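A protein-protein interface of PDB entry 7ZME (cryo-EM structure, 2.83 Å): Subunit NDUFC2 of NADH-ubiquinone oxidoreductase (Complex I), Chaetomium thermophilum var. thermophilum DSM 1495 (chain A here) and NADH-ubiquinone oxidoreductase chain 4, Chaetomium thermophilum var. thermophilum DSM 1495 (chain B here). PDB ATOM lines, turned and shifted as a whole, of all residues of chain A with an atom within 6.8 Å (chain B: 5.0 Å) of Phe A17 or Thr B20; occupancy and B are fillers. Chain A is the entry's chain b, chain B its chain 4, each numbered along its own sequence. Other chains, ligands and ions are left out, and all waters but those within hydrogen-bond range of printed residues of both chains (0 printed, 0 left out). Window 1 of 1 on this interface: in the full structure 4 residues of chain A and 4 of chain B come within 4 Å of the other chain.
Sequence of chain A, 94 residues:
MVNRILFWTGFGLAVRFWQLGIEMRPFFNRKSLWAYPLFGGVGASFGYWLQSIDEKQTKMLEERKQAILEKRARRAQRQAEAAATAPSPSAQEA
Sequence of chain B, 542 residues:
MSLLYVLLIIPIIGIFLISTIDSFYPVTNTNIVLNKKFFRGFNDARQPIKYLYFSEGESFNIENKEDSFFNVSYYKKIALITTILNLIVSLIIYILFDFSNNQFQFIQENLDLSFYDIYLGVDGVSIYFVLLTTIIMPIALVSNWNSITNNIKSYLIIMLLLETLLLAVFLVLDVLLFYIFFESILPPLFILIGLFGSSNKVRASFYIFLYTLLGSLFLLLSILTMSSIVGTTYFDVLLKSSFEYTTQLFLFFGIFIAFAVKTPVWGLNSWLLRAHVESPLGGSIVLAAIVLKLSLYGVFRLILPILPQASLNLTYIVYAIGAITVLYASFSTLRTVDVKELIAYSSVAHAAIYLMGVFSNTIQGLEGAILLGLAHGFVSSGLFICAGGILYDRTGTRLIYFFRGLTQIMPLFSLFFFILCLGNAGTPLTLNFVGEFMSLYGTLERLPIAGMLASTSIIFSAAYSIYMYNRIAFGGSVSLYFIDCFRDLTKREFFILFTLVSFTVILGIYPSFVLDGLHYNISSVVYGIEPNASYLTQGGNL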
ATOM      1  N   GLY A  12      13.834  -2.278  -6.284  1.00  0.00           N
ATOM      2  CA  GLY A  12      12.989  -3.454  -6.378  1.00  0.00           C
ATOM      3  C   GLY A  12      12.793  -3.927  -7.802  1.00  0.00           C
ATOM      4  O   GLY A  12      12.638  -5.126  -8.046  1.00  0.00           O
ATOM      5  N   LEU A  13      12.789  -2.997  -8.758  1.00  0.00           N
ATOM      6  CA  LEU A  13      12.694  -3.376 -10.163  1.00  0.00           C
ATOM      7  C   LEU A  13      13.912  -4.175 -10.601  1.00  0.00           C
ATOM      8  O   LEU A  13      13.787  -5.154 -11.345  1.00  0.00           O
ATOM      9  CB  LEU A  13      12.532  -2.130 -11.031  1.00  0.00           C
ATOM     10  CG  LEU A  13      11.228  -1.346 -10.888  1.00  0.00           C
ATOM     11  CD1 LEU A  13      11.290  -0.087 -11.725  1.00  0.00           C
ATOM     12  CD2 LEU A  13      10.044  -2.197 -11.282  1.00  0.00           C
ATOM     13  N   ALA A  14      15.103  -3.767 -10.154  1.00  0.00           N
ATOM     14  CA  ALA A  14      16.316  -4.480 -10.529  1.00  0.00           C
ATOM     15  C   ALA A  14      16.415  -5.829  -9.835  1.00  0.00           C
ATOM     16  O   ALA A  14      17.039  -6.752 -10.367  1.00  0.00           O
ATOM     17  CB  ALA A  14      17.544  -3.630 -10.215  1.00  0.00           C
ATOM     18  N   VAL A  15      15.827  -5.964  -8.646  1.00  0.00           N
ATOM     19  CA  VAL A  15      15.799  -7.266  -7.993  1.00  0.00           C
ATOM     20  C   VAL A  15      14.964  -8.244  -8.806  1.00  0.00           C
ATOM     21  O   VAL A  15      15.361  -9.394  -9.016  1.00  0.00           O
ATOM     22  CB  VAL A  15      15.282  -7.133  -6.550  1.00  0.00           C
ATOM     23  CG1 VAL A  15      15.070  -8.508  -5.932  1.00  0.00           C
ATOM     24  CG2 VAL A  15      16.249  -6.319  -5.711  1.00  0.00           C
ATOM     25  N   ARG A  16      13.802  -7.801  -9.285  1.00  0.00           N
ATOM     26  CA  ARG A  16      12.983  -8.645 -10.146  1.00  0.00           C
ATOM     27  C   ARG A  16      13.700  -8.960 -11.452  1.00  0.00           C
ATOM     28  O   ARG A  16      13.626 -10.085 -11.952  1.00  0.00           O
ATOM     29  CB  ARG A  16      11.643  -7.965 -10.413  1.00  0.00           C
ATOM     30  CG  ARG A  16      10.640  -8.817 -11.154  1.00  0.00           C
ATOM     31  CD  ARG A  16      10.485 -10.181 -10.536  1.00  0.00           C
ATOM     32  NE  ARG A  16       9.528 -10.976 -11.289  1.00  0.00           N
ATOM     33  CZ  ARG A  16       9.120 -12.188 -10.939  1.00  0.00           C
ATOM     34  NH1 ARG A  16       8.244 -12.832 -11.693  1.00  0.00           N
ATOM     35  NH2 ARG A  16       9.592 -12.755  -9.844  1.00  0.00           N
ATOM     36  N   PHE A  17      14.395  -7.973 -12.019  1.00  0.00           N
ATOM     37  CA  PHE A  17      15.169  -8.210 -13.233  1.00  0.00           C
ATOM     38  C   PHE A  17      16.290  -9.210 -12.983  1.00  0.00           C
ATOM     39  O   PHE A  17      16.448 -10.184 -13.725  1.00  0.00           O
ATOM     40  CB  PHE A  17      15.739  -6.892 -13.751  1.00  0.00           C
ATOM     41  CG  PHE A  17      16.097  -6.922 -15.202  1.00  0.00           C
ATOM     42  CD1 PHE A  17      15.115  -7.035 -16.169  1.00  0.00           C
ATOM     43  CD2 PHE A  17      17.420  -6.848 -15.601  1.00  0.00           C
ATOM     44  CE1 PHE A  17      15.443  -7.063 -17.506  1.00  0.00           C
ATOM     45  CE2 PHE A  17      17.755  -6.876 -16.933  1.00  0.00           C
ATOM     46  CZ  PHE A  17      16.766  -6.985 -17.889  1.00  0.00           C
ATOM     47  N   TRP A  18      17.084  -8.979 -11.937  1.00  0.00           N
ATOM     48  CA  TRP A  18      18.208  -9.863 -11.657  1.00  0.00           C
ATOM     49  C   TRP A  18      17.741 -11.255 -11.268  1.00  0.00           C
ATOM     50  O   TRP A  18      18.451 -12.236 -11.507  1.00  0.00           O
ATOM     51  CB  TRP A  18      19.075  -9.270 -10.552  1.00  0.00           C
ATOM     52  CG  TRP A  18      20.244  -8.511 -11.057  1.00  0.00           C
ATOM     53  CD1 TRP A  18      20.234  -7.263 -11.603  1.00  0.00           C
ATOM     54  CD2 TRP A  18      21.605  -8.945 -11.073  1.00  0.00           C
ATOM     55  NE1 TRP A  18      21.507  -6.890 -11.953  1.00  0.00           N
ATOM     56  CE2 TRP A  18      22.367  -7.907 -11.639  1.00  0.00           C
ATOM     57  CE3 TRP A  18      22.254 -10.110 -10.666  1.00  0.00           C
ATOM     58  CZ2 TRP A  18      23.744  -8.002 -11.809  1.00  0.00           C
ATOM     59  CZ3 TRP A  18      23.618 -10.198 -10.834  1.00  0.00           C
ATOM     60  CH2 TRP A  18      24.348  -9.153 -11.398  1.00  0.00           C
ATOM     61  N   GLN A  19      16.555 -11.359 -10.671  1.00  0.00           N
ATOM     62  CA  GLN A  19      16.057 -12.651 -10.217  1.00  0.00           C
ATOM     63  C   GLN A  19      15.651 -13.528 -11.390  1.00  0.00           C
ATOM     64  O   GLN A  19      15.913 -14.736 -11.389  1.00  0.00           O
ATOM     65  CB  GLN A  19      14.895 -12.430  -9.252  1.00  0.00           C
ATOM     66  CG  GLN A  19      14.423 -13.653  -8.524  1.00  0.00           C
ATOM     67  CD  GLN A  19      13.059 -14.105  -8.967  1.00  0.00           C
ATOM     68  OE1 GLN A  19      12.224 -13.296  -9.354  1.00  0.00           O
ATOM     69  NE2 GLN A  19      12.811 -15.401  -8.883  1.00  0.00           N
ATOM     70  N   LEU A  20      15.020 -12.940 -12.406  1.00  0.00           N
ATOM     71  CA  LEU A  20      14.661 -13.706 -13.592  1.00  0.00           C
ATOM     72  C   LEU A  20      15.889 -14.081 -14.406  1.00  0.00           C
ATOM     73  O   LEU A  20      15.916 -15.147 -15.030  1.00  0.00           O
ATOM     74  CB  LEU A  20      13.668 -12.917 -14.443  1.00  0.00           C
ATOM     75  CG  LEU A  20      12.393 -12.487 -13.712  1.00  0.00           C
ATOM     76  CD1 LEU A  20      11.475 -11.696 -14.623  1.00  0.00           C
ATOM     77  CD2 LEU A  20      11.676 -13.694 -13.140  1.00  0.00           C
ATOM     78  N   GLY A  21      16.912 -13.234 -14.386  1.00  0.00           N
ATOM     79  CA  GLY A  21      18.165 -13.571 -15.077  1.00  0.00           C
ATOM     80  C   GLY A  21      18.822 -14.768 -14.434  1.00  0.00           C
ATOM     81  O   GLY A  21      19.195 -15.691 -15.170  1.00  0.00           O
ATOM     82  N   ILE A  22      18.974 -14.755 -13.111  1.00  0.00           N
ATOM     83  CA  ILE A  22      19.618 -15.886 -12.384  1.00  0.00           C
ATOM     84  C   ILE A  22      18.825 -17.165 -12.650  1.00  0.00           C
ATOM     85  O   ILE A  22      19.452 -18.220 -12.763  1.00  0.00           O
ATOM     86  CB  ILE A  22      19.717 -15.604 -10.876  1.00  0.00           C
ATOM     87  CG1 ILE A  22      20.892 -14.681 -10.539  1.00  0.00           C
ATOM     88  CG2 ILE A  22      19.775 -16.902 -10.087  1.00  0.00           C
ATOM     89  CD1 ILE A  22      20.805 -14.076  -9.162  1.00  0.00           C
ATOM     90  N   ARG A  25      14.863 -17.141 -16.621  1.00  0.00           N
ATOM     91  CA  ARG A  25      13.456 -17.065 -17.072  1.00  0.00           C
ATOM     92  C   ARG A  25      13.292 -15.751 -17.850  1.00  0.00           C
ATOM     93  O   ARG A  25      13.912 -14.770 -17.433  1.00  0.00           O
ATOM     94  CB  ARG A  25      12.489 -17.087 -15.885  1.00  0.00           C
ATOM     95  CG  ARG A  25      12.067 -18.470 -15.418  1.00  0.00           C
ATOM     96  CD  ARG A  25      11.294 -18.320 -14.126  1.00  0.00           C
ATOM     97  NE  ARG A  25      10.324 -17.239 -14.224  1.00  0.00           N
ATOM     98  CZ  ARG A  25       9.672 -16.714 -13.195  1.00  0.00           C
ATOM     99  NH1 ARG A  25       8.809 -15.734 -13.391  1.00  0.00           N
ATOM    100  NH2 ARG A  25       9.891 -17.160 -11.972  1.00  0.00           N
ATOM    101  N   PHE A  27      12.529 -12.105 -19.064  1.00  0.00           N
ATOM    102  CA  PHE A  27      11.981 -10.884 -18.501  1.00  0.00           C
ATOM    103  C   PHE A  27      10.727 -10.490 -19.266  1.00  0.00           C
ATOM    104  O   PHE A  27      10.616 -10.708 -20.475  1.00  0.00           O
ATOM    105  CB  PHE A  27      12.981  -9.730 -18.564  1.00  0.00           C
ATOM    106  CG  PHE A  27      14.405 -10.124 -18.319  1.00  0.00           C
ATOM    107  CD1 PHE A  27      14.841 -10.456 -17.052  1.00  0.00           C
ATOM    108  CD2 PHE A  27      15.321 -10.115 -19.352  1.00  0.00           C
ATOM    109  CE1 PHE A  27      16.158 -10.798 -16.827  1.00  0.00           C
ATOM    110  CE2 PHE A  27      16.634 -10.457 -19.132  1.00  0.00           C
ATOM    111  CZ  PHE A  27      17.052 -10.796 -17.867  1.00  0.00           C
ATOM    112  N   PHE A  28       9.771  -9.916 -18.544  1.00  0.00           N
ATOM    113  CA  PHE A  28       8.578  -9.330 -19.149  1.00  0.00           C
ATOM    114  C   PHE A  28       7.722 -10.373 -19.858  1.00  0.00           C
ATOM    115  O   PHE A  28       7.297 -10.183 -20.998  1.00  0.00           O
ATOM    116  CB  PHE A  28       8.946  -8.187 -20.095  1.00  0.00           C
ATOM    117  CG  PHE A  28       9.985  -7.269 -19.541  1.00  0.00           C
ATOM    118  CD1 PHE A  28       9.811  -6.684 -18.301  1.00  0.00           C
ATOM    119  CD2 PHE A  28      11.138  -6.999 -20.244  1.00  0.00           C
ATOM    120  CE1 PHE A  28      10.764  -5.842 -17.779  1.00  0.00           C
ATOM    121  CE2 PHE A  28      12.088  -6.155 -19.722  1.00  0.00           C
ATOM    122  CZ  PHE A  28      11.900  -5.577 -18.490  1.00  0.00           C
ATOM    123  N   TYR A  36       6.533  -6.663 -11.248  1.00  0.00           N
ATOM    124  CA  TYR A  36       7.352  -5.459 -11.251  1.00  0.00           C
ATOM    125  C   TYR A  36       6.692  -4.365 -10.414  1.00  0.00           C
ATOM    126  O   TYR A  36       7.387  -3.680  -9.655  1.00  0.00           O
ATOM    127  CB  TYR A  36       7.633  -4.991 -12.682  1.00  0.00           C
ATOM    128  CG  TYR A  36       8.687  -5.821 -13.378  1.00  0.00           C
ATOM    129  CD1 TYR A  36      10.033  -5.610 -13.135  1.00  0.00           C
ATOM    130  CD2 TYR A  36       8.332  -6.826 -14.261  1.00  0.00           C
ATOM    131  CE1 TYR A  36      10.994  -6.369 -13.759  1.00  0.00           C
ATOM    132  CE2 TYR A  36       9.286  -7.587 -14.889  1.00  0.00           C
ATOM    133  CZ  TYR A  36      10.617  -7.357 -14.634  1.00  0.00           C
ATOM    134  OH  TYR A  36      11.574  -8.118 -15.259  1.00  0.00           O
ATOM    135  N   PHE A  39       7.385  -5.992  -6.749  1.00  0.00           N
ATOM    136  CA  PHE A  39       8.752  -5.791  -6.282  1.00  0.00           C
ATOM    137  C   PHE A  39       9.067  -4.313  -6.118  1.00  0.00           C
ATOM    138  O   PHE A  39       9.717  -3.922  -5.142  1.00  0.00           O
ATOM    139  CB  PHE A  39       9.744  -6.430  -7.253  1.00  0.00           C
ATOM    140  CG  PHE A  39       9.909  -7.915  -7.088  1.00  0.00           C
ATOM    141  CD1 PHE A  39       8.820  -8.766  -7.152  1.00  0.00           C
ATOM    142  CD2 PHE A  39      11.161  -8.460  -6.885  1.00  0.00           C
ATOM    143  CE1 PHE A  39       8.977 -10.129  -7.014  1.00  0.00           C
ATOM    144  CE2 PHE A  39      11.324  -9.822  -6.750  1.00  0.00           C
ATOM    145  CZ  PHE A  39      10.228 -10.657  -6.814  1.00  0.00           C
ATOM    146  N   PHE B  16      21.090  -1.381 -20.613  1.00  0.00           N
ATOM    147  CA  PHE B  16      19.727  -1.849 -20.388  1.00  0.00           C
ATOM    148  C   PHE B  16      19.059  -2.261 -21.690  1.00  0.00           C
ATOM    149  O   PHE B  16      18.412  -3.312 -21.755  1.00  0.00           O
ATOM    150  CB  PHE B  16      18.901  -0.772 -19.690  1.00  0.00           C
ATOM    151  CG  PHE B  16      17.539  -1.237 -19.274  1.00  0.00           C
ATOM    152  CD1 PHE B  16      17.371  -2.470 -18.665  1.00  0.00           C
ATOM    153  CD2 PHE B  16      16.423  -0.450 -19.496  1.00  0.00           C
ATOM    154  CE1 PHE B  16      16.117  -2.908 -18.282  1.00  0.00           C
ATOM    155  CE2 PHE B  16      15.166  -0.878 -19.115  1.00  0.00           C
ATOM    156  CZ  PHE B  16      15.013  -2.109 -18.509  1.00  0.00           C
ATOM    157  N   LEU B  17      19.196  -1.450 -22.739  1.00  0.00           N
ATOM    158  CA  LEU B  17      18.569  -1.789 -24.012  1.00  0.00           C
ATOM    159  C   LEU B  17      19.148  -3.076 -24.587  1.00  0.00           C
ATOM    160  O   LEU B  17      18.404  -3.961 -25.018  1.00  0.00           O
ATOM    161  CB  LEU B  17      18.724  -0.640 -25.005  1.00  0.00           C
ATOM    162  CG  LEU B  17      18.052   0.676 -24.621  1.00  0.00           C
ATOM    163  CD1 LEU B  17      18.503   1.794 -25.547  1.00  0.00           C
ATOM    164  CD2 LEU B  17      16.544   0.525 -24.642  1.00  0.00           C
ATOM    165  N   ILE B  18      20.474  -3.211 -24.574  1.00  0.00           N
ATOM    166  CA  ILE B  18      21.107  -4.380 -25.179  1.00  0.00           C
ATOM    167  C   ILE B  18      20.669  -5.657 -24.474  1.00  0.00           C
ATOM    168  O   ILE B  18      20.401  -6.680 -25.116  1.00  0.00           O
ATOM    169  CB  ILE B  18      22.638  -4.218 -25.170  1.00  0.00           C
ATOM    170  CG1 ILE B  18      23.073  -3.235 -26.260  1.00  0.00           C
ATOM    171  CG2 ILE B  18      23.322  -5.557 -25.358  1.00  0.00           C
ATOM    172  CD1 ILE B  18      24.477  -2.695 -26.076  1.00  0.00           C
ATOM    173  N   SER B  19      20.572  -5.618 -23.149  1.00  0.00           N
ATOM    174  CA  SER B  19      20.237  -6.811 -22.385  1.00  0.00           C
ATOM    175  C   SER B  19      18.747  -7.127 -22.383  1.00  0.00           C
ATOM    176  O   SER B  19      18.356  -8.174 -21.856  1.00  0.00           O
ATOM    177  CB  SER B  19      20.728  -6.660 -20.946  1.00  0.00           C
ATOM    178  OG  SER B  19      20.393  -5.387 -20.428  1.00  0.00           O
ATOM    179  N   THR B  20      17.912  -6.266 -22.959  1.00  0.00           N
ATOM    180  CA  THR B  20      16.470  -6.390 -22.818  1.00  0.00           C
ATOM    181  C   THR B  20      15.734  -6.579 -24.142  1.00  0.00           C
ATOM    182  O   THR B  20      14.600  -7.068 -24.130  1.00  0.00           O
ATOM    183  CB  THR B  20      15.933  -5.153 -22.078  1.00  0.00           C
ATOM    184  OG1 THR B  20      16.546  -5.078 -20.788  1.00  0.00           O
ATOM    185  CG2 THR B  20      14.448  -5.225 -21.869  1.00  0.00           C
ATOM    186  N   ILE B  21      16.356  -6.261 -25.282  1.00  0.00           N
ATOM    187  CA  ILE B  21      15.670  -6.406 -26.567  1.00  0.00           C
ATOM    188  C   ILE B  21      15.239  -7.849 -26.794  1.00  0.00           C
ATOM    189  O   ILE B  21      14.153  -8.111 -27.326  1.00  0.00           O
ATOM    190  CB  ILE B  21      16.548  -5.896 -27.724  1.00  0.00           C
ATOM    191  CG1 ILE B  21      16.903  -4.426 -27.530  1.00  0.00           C
ATOM    192  CG2 ILE B  21      15.849  -6.090 -29.058  1.00  0.00           C
ATOM    193  CD1 ILE B  21      15.701  -3.512 -27.495  1.00  0.00           C
ATOM    194  N   ASP B  22      16.082  -8.807 -26.402  1.00  0.00           N
ATOM    195  CA  ASP B  22      15.732 -10.214 -26.566  1.00  0.00           C
ATOM    196  C   ASP B  22      14.385 -10.529 -25.926  1.00  0.00           C
ATOM    197  O   ASP B  22      13.614 -11.344 -26.447  1.00  0.00           O
ATOM    198  CB  ASP B  22      16.828 -11.098 -25.972  1.00  0.00           C
ATOM    199  CG  ASP B  22      16.782 -12.516 -26.502  1.00  0.00           C
ATOM    200  OD1 ASP B  22      15.990 -12.780 -27.430  1.00  0.00           O
ATOM    201  OD2 ASP B  22      17.537 -13.369 -25.988  1.00  0.00           O
ATOM    202  N   SER B  23      14.082  -9.891 -24.795  1.00  0.00           N
ATOM    203  CA  SER B  23      12.780 -10.071 -24.165  1.00  0.00           C
ATOM    204  C   SER B  23      11.691  -9.274 -24.876  1.00  0.00           C
ATOM    205  O   SER B  23      10.544  -9.728 -24.960  1.00  0.00           O
ATOM    206  CB  SER B  23      12.851  -9.675 -22.691  1.00  0.00           C
ATOM    207  OG  SER B  23      13.024  -8.278 -22.552  1.00  0.00           O
ATOM    208  N   PHE B  24      12.028  -8.087 -25.390  1.00  0.00           N
ATOM    209  CA  PHE B  24      11.019  -7.239 -26.016  1.00  0.00           C
ATOM    210  C   PHE B  24      10.474  -7.871 -27.294  1.00  0.00           C
ATOM    211  O   PHE B  24       9.256  -7.970 -27.477  1.00  0.00           O
ATOM    212  CB  PHE B  24      11.596  -5.854 -26.307  1.00  0.00           C
ATOM    213  CG  PHE B  24      11.342  -4.852 -25.217  1.00  0.00           C
ATOM    214  CD1 PHE B  24      10.046  -4.512 -24.863  1.00  0.00           C
ATOM    215  CD2 PHE B  24      12.392  -4.236 -24.558  1.00  0.00           C
ATOM    216  CE1 PHE B  24       9.803  -3.587 -23.865  1.00  0.00           C
ATOM    217  CE2 PHE B  24      12.155  -3.307 -23.560  1.00  0.00           C
ATOM    218  CZ  PHE B  24      10.860  -2.984 -23.213  1.00  0.00           C
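Hydrophobic or aromatic side chains of chain A within 4 Å of the printed part of chain B: Phe A17, Phe A27 and Phe A28.
Among the printed residues, no Asp or Glu carboxylate lies within 4 Å of a Lys or Arg side-chain nitrogen of the other chain.
The side-chain hydroxyl (OG1) of Thr B20 lies within hydrogen-bond range of the backbone carbonyl oxygen (O) of Phe B16.
OG of Ser B23 sits at hydrogen-bond distance from O of Thr B20, at 2.5 Å.
The side-chain hydroxyl (OG) of Ser B19 sits at hydrogen-bond distance from the backbone carbonyl oxygen (O) of Phe B16 (3.2 Å).
Among the printed residues, merely in contact across the chains: Phe A17 with Thr B20, Phe A27 with Ser B19, Phe A27 with Ser B23, Phe A28 with Thr B20 and Phe A28 with Ser B23.
Phe A17 touches just one residue of chain B: Thr B20.
Of the printed residues of chain B, Phe A27 touches Ser B19 and Ser B23.
Printed residues of chain B within 4 Å of Phe A28: Thr B20 (3.3 Å) and Ser B23 (3.2 Å).
Of the printed residues of chain A, Ser B19 touches Phe A27.
Of chain A, only Phe A17 (3.5 Å) and Phe A28 (3.3 Å) come within 4 Å of Thr B20.
Phe B24 touches none of the printed residues of chain A.
The nearest residue of chain B that does not touch Phe A17 is Phe B16 (4.1 Å).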
